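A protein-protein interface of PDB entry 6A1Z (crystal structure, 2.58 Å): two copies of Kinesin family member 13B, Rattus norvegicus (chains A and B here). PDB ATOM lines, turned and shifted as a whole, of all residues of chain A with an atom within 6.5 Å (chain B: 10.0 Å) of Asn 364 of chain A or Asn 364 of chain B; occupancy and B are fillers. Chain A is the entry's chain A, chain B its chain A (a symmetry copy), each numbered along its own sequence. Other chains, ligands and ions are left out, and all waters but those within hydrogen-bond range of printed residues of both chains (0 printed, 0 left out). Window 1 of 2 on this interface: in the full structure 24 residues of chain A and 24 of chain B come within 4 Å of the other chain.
ND2 of Asn 364 of chain A lies within hydrogen-bond range of OD2 of Asp 362 of chain B (3.2 Å). OD2 of Asp 362 of chain A lies within hydrogen-bond range of ND2 of Asn 364 of chain B, 3.2 Å away.
The side-chain carboxylate of Asp 362 of chain B lies within hydrogen-bond range of the backbone NH of Asn 364 of chain B (3.0 Å). The side-chain carboxylate (OD1) of Asp 362 of chain A sits at hydrogen-bond distance from the backbone NH (N) of Asn 364 of chain A.
Among the printed residues, merely in contact across the chains: Asn 364 of chain A with Asn 364 of chain B, Asn 364 of chain A with Ala 365 of chain B, Asn 364 of chain A with Ile 368 of chain B, Ala 365 of chain A with Asn 364 of chain B, Ile 367 of chain A with Ile 368 of chain B, Ile 367 of chain A with Arg 372 of chain B, Ile 368 of chain A with Asn 364 of chain B, Ile 368 of chain A with Ile 367 of chain B, Ile 368 of chain A with Ile 368 of chain B and Ile 368 of chain A with Leu 371 of chain B.
Asp 362 of chain A touches just one residue of chain B: Asn 364 (3.2 Å). Asn 364 of chain A touches four residues of chain B. Of chain B, only Asn 364 comes within 4 Å of Ala 365 of chain A. Of the printed residues of chain B, Ile 367 of chain A touches Ile 368 and Arg 372. Of the printed residues of chain B, Ile 368 of chain A touches Asn 364 (3.5 Å), Ile 367 (3.8 Å), Ile 368 (3.4 Å) and Leu 371 (3.8 Å). Gly 243 of chain B touches none of the printed residues of chain A. Printed residues of chain A within 4 Å of Ala 365 of chain B: Asn 364 (3.9 Å). The nearest residue of chain B that does not touch Asn 364 of chain A is Pro 363 of chain B (6.4 Å). The nearest residue of chain A that does not touch Asn 364 of chain B is Pro 363 of chain A (6.4 Å). The nearest printed residue of chain A that does not touch Leu 371 of chain B is Ile 367 of chain A (5.4 Å).
Of the 19 printed residues of chain B, 7 touch a printed residue of chain A. Hydrophobic or aromatic side chains of chain B within 4 Å of the printed part of chain A: Ile 367, Ile 368 and Leu 371. Of the 9 printed residues of chain A, 5 touch a printed residue of chain B. Along chain A the printed residues that touch a printed residue of chain B span positions 362 to 368. Among the printed residues, no Asp or Glu carboxylate lies within 4 Å of a Lys or Arg side-chain nitrogen of the other chain.
Asp 362 of chain A touches Asn 364 of chain B, and with the chains exchanged Asn 364 of chain A touches Asp 362 of chain B. Asn 364 of chain A touches its own counterpart, Asn 364 of chain B. Ile 367 of chain A touches Ile 368 of chain B, and with the chains exchanged Ile 368 of chain A touches Ile 367 of chain B. Ile 368 of chain A touches its own counterpart, Ile 368 of chain B. Of the 12 pairs that touch across the chains among the printed residues, 10 have their exchanged pair printed and touching as well.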
ATOM      1  N   GLU A 361     -14.179 -39.298   5.265  1.00  0.00           N
ATOM      2  CA  GLU A 361     -14.815 -38.867   4.030  1.00  0.00           C
ATOM      3  C   GLU A 361     -13.890 -37.876   3.316  1.00  0.00           C
ATOM      4  O   GLU A 361     -12.708 -37.738   3.658  1.00  0.00           O
ATOM      5  CB  GLU A 361     -16.193 -38.234   4.334  1.00  0.00           C
ATOM      6  CG  GLU A 361     -17.333 -39.234   4.738  1.00  0.00           C
ATOM      7  CD  GLU A 361     -18.580 -39.240   3.814  1.00  0.00           C
ATOM      8  OE1 GLU A 361     -18.455 -39.495   2.589  1.00  0.00           O
ATOM      9  OE2 GLU A 361     -19.706 -39.050   4.334  1.00  0.00           O
ATOM     10  N   ASP A 362     -14.445 -37.143   2.337  1.00  0.00           N
ATOM     11  CA  ASP A 362     -13.681 -36.176   1.547  1.00  0.00           C
ATOM     12  C   ASP A 362     -13.816 -34.772   2.137  1.00  0.00           C
ATOM     13  O   ASP A 362     -14.941 -34.268   2.244  1.00  0.00           O
ATOM     14  CB  ASP A 362     -14.165 -36.188   0.101  1.00  0.00           C
ATOM     15  CG  ASP A 362     -13.466 -35.161  -0.792  1.00  0.00           C
ATOM     16  OD1 ASP A 362     -12.395 -34.616  -0.415  1.00  0.00           O
ATOM     17  OD2 ASP A 362     -14.023 -34.890  -1.887  1.00  0.00           O
ATOM     18  N   PRO A 363     -12.712 -34.113   2.503  1.00  0.00           N
ATOM     19  CA  PRO A 363     -12.793 -32.703   2.933  1.00  0.00           C
ATOM     20  C   PRO A 363     -13.601 -31.810   1.996  1.00  0.00           C
ATOM     21  O   PRO A 363     -14.294 -30.900   2.466  1.00  0.00           O
ATOM     22  CB  PRO A 363     -11.320 -32.265   2.958  1.00  0.00           C
ATOM     23  CG  PRO A 363     -10.537 -33.512   3.045  1.00  0.00           C
ATOM     24  CD  PRO A 363     -11.328 -34.613   2.458  1.00  0.00           C
ATOM     25  N   ASN A 364     -13.533 -32.052   0.681  1.00  0.00           N
ATOM     26  CA  ASN A 364     -14.058 -31.092  -0.288  1.00  0.00           C
ATOM     27  C   ASN A 364     -15.572 -30.972  -0.203  1.00  0.00           C
ATOM     28  O   ASN A 364     -16.114 -29.861  -0.231  1.00  0.00           O
ATOM     29  CB  ASN A 364     -13.627 -31.490  -1.695  1.00  0.00           C
ATOM     30  CG  ASN A 364     -12.199 -31.085  -1.993  1.00  0.00           C
ATOM     31  OD1 ASN A 364     -11.507 -30.534  -1.130  1.00  0.00           O
ATOM     32  ND2 ASN A 364     -11.748 -31.346  -3.222  1.00  0.00           N
ATOM     33  N   ALA A 365     -16.276 -32.108  -0.099  1.00  0.00           N
ATOM     34  CA  ALA A 365     -17.739 -32.091  -0.147  1.00  0.00           C
ATOM     35  C   ALA A 365     -18.339 -31.121   0.872  1.00  0.00           C
ATOM     36  O   ALA A 365     -19.255 -30.354   0.548  1.00  0.00           O
ATOM     37  CB  ALA A 365     -18.292 -33.498   0.070  1.00  0.00           C
ATOM     38  N   ARG A 366     -17.822 -31.128   2.105  1.00  0.00           N
ATOM     39  CA  ARG A 366     -18.305 -30.191   3.115  1.00  0.00           C
ATOM     40  C   ARG A 366     -17.856 -28.754   2.825  1.00  0.00           C
ATOM     41  O   ARG A 366     -18.569 -27.797   3.147  1.00  0.00           O
ATOM     42  CB  ARG A 366     -17.839 -30.644   4.490  1.00  0.00           C
ATOM     43  CG  ARG A 366     -17.915 -29.546   5.529  1.00  0.00           C
ATOM     44  CD  ARG A 366     -17.667 -30.050   6.927  1.00  0.00           C
ATOM     45  NE  ARG A 366     -18.874 -30.635   7.493  1.00  0.00           N
ATOM     46  CZ  ARG A 366     -18.912 -31.264   8.660  1.00  0.00           C
ATOM     47  NH1 ARG A 366     -17.801 -31.380   9.382  1.00  0.00           N
ATOM     48  NH2 ARG A 366     -20.059 -31.772   9.103  1.00  0.00           N
ATOM     49  N   ILE A 367     -16.689 -28.574   2.203  1.00  0.00           N
ATOM     50  CA  ILE A 367     -16.247 -27.230   1.828  1.00  0.00           C
ATOM     51  C   ILE A 367     -17.168 -26.641   0.762  1.00  0.00           C
ATOM     52  O   ILE A 367     -17.489 -25.446   0.780  1.00  0.00           O
ATOM     53  CB  ILE A 367     -14.780 -27.261   1.356  1.00  0.00           C
ATOM     54  CG1 ILE A 367     -13.839 -27.551   2.530  1.00  0.00           C
ATOM     55  CG2 ILE A 367     -14.423 -25.949   0.698  1.00  0.00           C
ATOM     56  CD1 ILE A 367     -12.420 -27.948   2.115  1.00  0.00           C
ATOM     57  N   ILE A 368     -17.589 -27.459  -0.198  1.00  0.00           N
ATOM     58  CA  ILE A 368     -18.542 -26.965  -1.172  1.00  0.00           C
ATOM     59  C   ILE A 368     -19.848 -26.597  -0.480  1.00  0.00           C
ATOM     60  O   ILE A 368     -20.406 -25.520  -0.710  1.00  0.00           O
ATOM     61  CB  ILE A 368     -18.747 -28.004  -2.283  1.00  0.00           C
ATOM     62  CG1 ILE A 368     -17.504 -28.062  -3.187  1.00  0.00           C
ATOM     63  CG2 ILE A 368     -20.006 -27.686  -3.058  1.00  0.00           C
ATOM     64  CD1 ILE A 368     -17.266 -29.431  -3.852  1.00  0.00           C
ATOM     65  N   ARG A 369     -20.316 -27.462   0.421  1.00  0.00           N
ATOM     66  CA  ARG A 369     -21.608 -27.262   1.069  1.00  0.00           C
ATOM     67  C   ARG A 369     -21.669 -25.924   1.784  1.00  0.00           C
ATOM     68  O   ARG A 369     -22.659 -25.190   1.685  1.00  0.00           O
ATOM     69  CB  ARG A 369     -21.877 -28.399   2.050  1.00  0.00           C
ATOM     70  CG  ARG A 369     -22.793 -29.433   1.494  1.00  0.00           C
ATOM     71  CD  ARG A 369     -23.177 -30.396   2.548  1.00  0.00           C
ATOM     72  NE  ARG A 369     -22.446 -31.651   2.418  1.00  0.00           N
ATOM     73  CZ  ARG A 369     -21.567 -32.113   3.305  1.00  0.00           C
ATOM     74  NH1 ARG A 369     -21.286 -31.423   4.401  1.00  0.00           N
ATOM     75  NH2 ARG A 369     -20.968 -33.273   3.086  1.00  0.00           N
ATOM     76  N   SER B 239      -0.476 -27.623   2.192  1.00  0.00           N
ATOM     77  CA  SER B 239      -1.889 -27.602   2.551  1.00  0.00           C
ATOM     78  C   SER B 239      -2.333 -28.848   3.318  1.00  0.00           C
ATOM     79  O   SER B 239      -3.413 -28.831   3.911  1.00  0.00           O
ATOM     80  CB  SER B 239      -2.753 -27.420   1.300  1.00  0.00           C
ATOM     81  N   GLY B 240      -1.528 -29.915   3.335  1.00  0.00           N
ATOM     82  CA  GLY B 240      -1.893 -31.134   4.040  1.00  0.00           C
ATOM     83  C   GLY B 240      -2.978 -31.967   3.391  1.00  0.00           C
ATOM     84  O   GLY B 240      -3.530 -32.860   4.039  1.00  0.00           O
ATOM     85  N   THR B 241      -3.295 -31.715   2.123  1.00  0.00           N
ATOM     86  CA  THR B 241      -4.382 -32.377   1.415  1.00  0.00           C
ATOM     87  C   THR B 241      -3.836 -33.331   0.345  1.00  0.00           C
ATOM     88  O   THR B 241      -2.629 -33.405   0.087  1.00  0.00           O
ATOM     89  CB  THR B 241      -5.317 -31.326   0.810  1.00  0.00           C
ATOM     90  N   SER B 242      -4.728 -34.097  -0.276  1.00  0.00           N
ATOM     91  CA  SER B 242      -4.274 -35.059  -1.274  1.00  0.00           C
ATOM     92  C   SER B 242      -5.275 -35.169  -2.414  1.00  0.00           C
ATOM     93  O   SER B 242      -6.486 -35.207  -2.185  1.00  0.00           O
ATOM     94  CB  SER B 242      -4.059 -36.448  -0.667  1.00  0.00           C
ATOM     95  OG  SER B 242      -5.307 -37.095  -0.467  1.00  0.00           O
ATOM     96  N   GLY B 243      -4.752 -35.238  -3.643  1.00  0.00           N
ATOM     97  CA  GLY B 243      -5.559 -35.523  -4.805  1.00  0.00           C
ATOM     98  C   GLY B 243      -4.980 -36.697  -5.598  1.00  0.00           C
ATOM     99  O   GLY B 243      -3.839 -37.114  -5.389  1.00  0.00           O
ATOM    100  N   GLU B 244      -5.807 -37.206  -6.507  1.00  0.00           N
ATOM    101  CA  GLU B 244      -5.491 -38.382  -7.319  1.00  0.00           C
ATOM    102  C   GLU B 244      -5.832 -38.083  -8.775  1.00  0.00           C
ATOM    103  O   GLU B 244      -6.967 -37.706  -9.086  1.00  0.00           O
ATOM    104  CB  GLU B 244      -6.246 -39.632  -6.812  1.00  0.00           C
ATOM    105  CG  GLU B 244      -7.791 -39.520  -6.630  1.00  0.00           C
ATOM    106  CD  GLU B 244      -8.249 -38.502  -5.547  1.00  0.00           C
ATOM    107  OE1 GLU B 244      -8.998 -37.559  -5.904  1.00  0.00           O
ATOM    108  OE2 GLU B 244      -7.875 -38.639  -4.350  1.00  0.00           O
ATOM    109  N   ASN B 360      -8.004 -36.294 -16.012  1.00  0.00           N
ATOM    110  CA  ASN B 360      -9.012 -36.855 -15.118  1.00  0.00           C
ATOM    111  C   ASN B 360      -8.604 -36.539 -13.687  1.00  0.00           C
ATOM    112  O   ASN B 360      -8.011 -37.351 -12.973  1.00  0.00           O
ATOM    113  CB  ASN B 360      -9.179 -38.346 -15.367  1.00  0.00           C
ATOM    114  CG  ASN B 360      -9.123 -38.696 -16.846  1.00  0.00           C
ATOM    115  OD1 ASN B 360      -9.917 -38.196 -17.660  1.00  0.00           O
ATOM    116  ND2 ASN B 360      -8.159 -39.533 -17.207  1.00  0.00           N
ATOM    117  N   GLU B 361      -8.935 -35.309 -13.283  1.00  0.00           N
ATOM    118  CA  GLU B 361      -8.738 -34.743 -11.959  1.00  0.00           C
ATOM    119  C   GLU B 361     -10.044 -34.871 -11.166  1.00  0.00           C
ATOM    120  O   GLU B 361     -10.968 -35.594 -11.561  1.00  0.00           O
ATOM    121  CB  GLU B 361      -8.291 -33.267 -12.072  1.00  0.00           C
ATOM    122  CG  GLU B 361      -6.813 -33.032 -12.545  1.00  0.00           C
ATOM    123  CD  GLU B 361      -5.904 -32.261 -11.552  1.00  0.00           C
ATOM    124  OE1 GLU B 361      -5.720 -32.706 -10.390  1.00  0.00           O
ATOM    125  OE2 GLU B 361      -5.316 -31.231 -11.961  1.00  0.00           O
ATOM    126  N   ASP B 362     -10.141 -34.125 -10.054  1.00  0.00           N
ATOM    127  CA  ASP B 362     -11.315 -34.163  -9.180  1.00  0.00           C
ATOM    128  C   ASP B 362     -12.292 -33.044  -9.542  1.00  0.00           C
ATOM    129  O   ASP B 362     -11.908 -31.869  -9.497  1.00  0.00           O
ATOM    130  CB  ASP B 362     -10.883 -34.034  -7.723  1.00  0.00           C
ATOM    131  CG  ASP B 362     -12.050 -33.999  -6.734  1.00  0.00           C
ATOM    132  OD1 ASP B 362     -13.199 -34.366  -7.095  1.00  0.00           O
ATOM    133  OD2 ASP B 362     -11.799 -33.576  -5.576  1.00  0.00           O
ATOM    134  N   PRO B 363     -13.547 -33.362  -9.878  1.00  0.00           N
ATOM    135  CA  PRO B 363     -14.554 -32.303 -10.084  1.00  0.00           C
ATOM    136  C   PRO B 363     -14.601 -31.260  -8.972  1.00  0.00           C
ATOM    137  O   PRO B 363     -14.831 -30.076  -9.253  1.00  0.00           O
ATOM    138  CB  PRO B 363     -15.874 -33.090 -10.141  1.00  0.00           C
ATOM    139  CG  PRO B 363     -15.495 -34.477 -10.466  1.00  0.00           C
ATOM    140  CD  PRO B 363     -14.113 -34.715 -10.000  1.00  0.00           C
ATOM    141  N   ASN B 364     -14.382 -31.668  -7.715  1.00  0.00           N
ATOM    142  CA  ASN B 364     -14.667 -30.792  -6.581  1.00  0.00           C
ATOM    143  C   ASN B 364     -13.736 -29.589  -6.546  1.00  0.00           C
ATOM    144  O   ASN B 364     -14.182 -28.459  -6.316  1.00  0.00           O
ATOM    145  CB  ASN B 364     -14.574 -31.583  -5.281  1.00  0.00           C
ATOM    146  CG  ASN B 364     -15.816 -32.407  -5.022  1.00  0.00           C
ATOM    147  OD1 ASN B 364     -16.746 -32.420  -5.836  1.00  0.00           O
ATOM    148  ND2 ASN B 364     -15.850 -33.096  -3.878  1.00  0.00           N
ATOM    149  N   ALA B 365     -12.434 -29.810  -6.772  1.00  0.00           N
ATOM    150  CA  ALA B 365     -11.453 -28.733  -6.626  1.00  0.00           C
ATOM    151  C   ALA B 365     -11.826 -27.497  -7.446  1.00  0.00           C
ATOM    152  O   ALA B 365     -11.748 -26.365  -6.950  1.00  0.00           O
ATOM    153  CB  ALA B 365     -10.061 -29.228  -7.015  1.00  0.00           C
ATOM    154  N   ARG B 366     -12.253 -27.695  -8.697  1.00  0.00           N
ATOM    155  CA  ARG B 366     -12.680 -26.569  -9.520  1.00  0.00           C
ATOM    156  C   ARG B 366     -14.019 -25.988  -9.048  1.00  0.00           C
ATOM    157  O   ARG B 366     -14.259 -24.783  -9.175  1.00  0.00           O
ATOM    158  CB  ARG B 366     -12.754 -27.004 -10.975  1.00  0.00           C
ATOM    159  CG  ARG B 366     -13.577 -26.064 -11.830  1.00  0.00           C
ATOM    160  CD  ARG B 366     -13.467 -26.370 -13.302  1.00  0.00           C
ATOM    161  NE  ARG B 366     -12.259 -25.786 -13.868  1.00  0.00           N
ATOM    162  CZ  ARG B 366     -11.849 -26.001 -15.111  1.00  0.00           C
ATOM    163  NH1 ARG B 366     -12.564 -26.785 -15.915  1.00  0.00           N
ATOM    164  NH2 ARG B 366     -10.730 -25.430 -15.548  1.00  0.00           N
ATOM    165  N   ILE B 367     -14.898 -26.819  -8.485  1.00  0.00           N
ATOM    166  CA  ILE B 367     -16.158 -26.308  -7.942  1.00  0.00           C
ATOM    167  C   ILE B 367     -15.897 -25.402  -6.741  1.00  0.00           C
ATOM    168  O   ILE B 367     -16.557 -24.372  -6.558  1.00  0.00           O
ATOM    169  CB  ILE B 367     -17.097 -27.475  -7.578  1.00  0.00           C
ATOM    170  CG1 ILE B 367     -17.599 -28.182  -8.842  1.00  0.00           C
ATOM    171  CG2 ILE B 367     -18.257 -26.967  -6.755  1.00  0.00           C
ATOM    172  CD1 ILE B 367     -18.240 -29.547  -8.587  1.00  0.00           C
ATOM    173  N   ILE B 368     -14.948 -25.780  -5.889  1.00  0.00           N
ATOM    174  CA  ILE B 368     -14.602 -24.900  -4.791  1.00  0.00           C
ATOM    175  C   ILE B 368     -14.034 -23.594  -5.331  1.00  0.00           C
ATOM    176  O   ILE B 368     -14.430 -22.505  -4.907  1.00  0.00           O
ATOM    177  CB  ILE B 368     -13.627 -25.606  -3.838  1.00  0.00           C
ATOM    178  CG1 ILE B 368     -14.366 -26.692  -3.037  1.00  0.00           C
ATOM    179  CG2 ILE B 368     -12.956 -24.588  -2.942  1.00  0.00           C
ATOM    180  CD1 ILE B 368     -13.479 -27.873  -2.603  1.00  0.00           C
ATOM    181  N   ARG B 369     -13.142 -23.689  -6.320  1.00  0.00           N
ATOM    182  CA  ARG B 369     -12.458 -22.512  -6.843  1.00  0.00           C
ATOM    183  C   ARG B 369     -13.445 -21.473  -7.343  1.00  0.00           C
ATOM    184  O   ARG B 369     -13.307 -20.275  -7.070  1.00  0.00           O
ATOM    185  CB  ARG B 369     -11.507 -22.921  -7.963  1.00  0.00           C
ATOM    186  CG  ARG B 369     -10.092 -23.018  -7.510  1.00  0.00           C
ATOM    187  CD  ARG B 369      -9.195 -23.216  -8.669  1.00  0.00           C
ATOM    188  NE  ARG B 369      -8.762 -24.604  -8.778  1.00  0.00           N
ATOM    189  CZ  ARG B 369      -9.076 -25.421  -9.780  1.00  0.00           C
ATOM    190  NH1 ARG B 369      -9.846 -25.006 -10.777  1.00  0.00           N
ATOM    191  NH2 ARG B 369      -8.616 -26.663  -9.778  1.00  0.00           N
ATOM    192  N   ASP B 370     -14.452 -21.916  -8.076  1.00  0.00           N
ATOM    193  CA  ASP B 370     -15.401 -20.965  -8.626  1.00  0.00           C
ATOM    194  C   ASP B 370     -16.387 -20.473  -7.569  1.00  0.00           C
ATOM    195  O   ASP B 370     -16.870 -19.339  -7.660  1.00  0.00           O
ATOM    196  CB  ASP B 370     -16.089 -21.607  -9.828  1.00  0.00           C
ATOM    197  CG  ASP B 370     -15.122 -21.797 -11.020  1.00  0.00           C
ATOM    198  OD1 ASP B 370     -14.413 -22.829 -11.075  1.00  0.00           O
ATOM    199  OD2 ASP B 370     -15.069 -20.909 -11.911  1.00  0.00           O
ATOM    200  N   LEU B 371     -16.671 -21.283  -6.544  1.00  0.00           N
ATOM    201  CA  LEU B 371     -17.530 -20.823  -5.460  1.00  0.00           C
ATOM    202  C   LEU B 371     -16.850 -19.733  -4.646  1.00  0.00           C
ATOM    203  O   LEU B 371     -17.490 -18.759  -4.242  1.00  0.00           O
ATOM    204  CB  LEU B 371     -17.912 -21.993  -4.560  1.00  0.00           C
ATOM    205  CG  LEU B 371     -19.065 -22.876  -5.028  1.00  0.00           C
ATOM    206  CD1 LEU B 371     -19.140 -24.132  -4.160  1.00  0.00           C
ATOM    207  CD2 LEU B 371     -20.382 -22.100  -5.012  1.00  0.00           C
ATOM    208  N   ARG B 372     -15.549 -19.882  -4.400  1.00  0.00           N
ATOM    209  CA  ARG B 372     -14.810 -18.893  -3.623  1.00  0.00           C
ATOM    210  C   ARG B 372     -14.748 -17.547  -4.332  1.00  0.00           C
ATOM    211  O   ARG B 372     -14.730 -16.491  -3.685  1.00  0.00           O
ATOM    212  CB  ARG B 372     -13.400 -19.404  -3.367  1.00  0.00           C
ATOM    213  CG  ARG B 372     -13.332 -20.652  -2.512  1.00  0.00           C
ATOM    214  CD  ARG B 372     -12.142 -20.572  -1.590  1.00  0.00           C
ATOM    215  NE  ARG B 372     -12.187 -21.578  -0.541  1.00  0.00           N
ATOM    216  CZ  ARG B 372     -11.250 -22.505  -0.366  1.00  0.00           C
ATOM    217  NH1 ARG B 372     -10.204 -22.539  -1.182  1.00  0.00           N
ATOM    218  NH2 ARG B 372     -11.356 -23.393   0.625  1.00  0.00           N
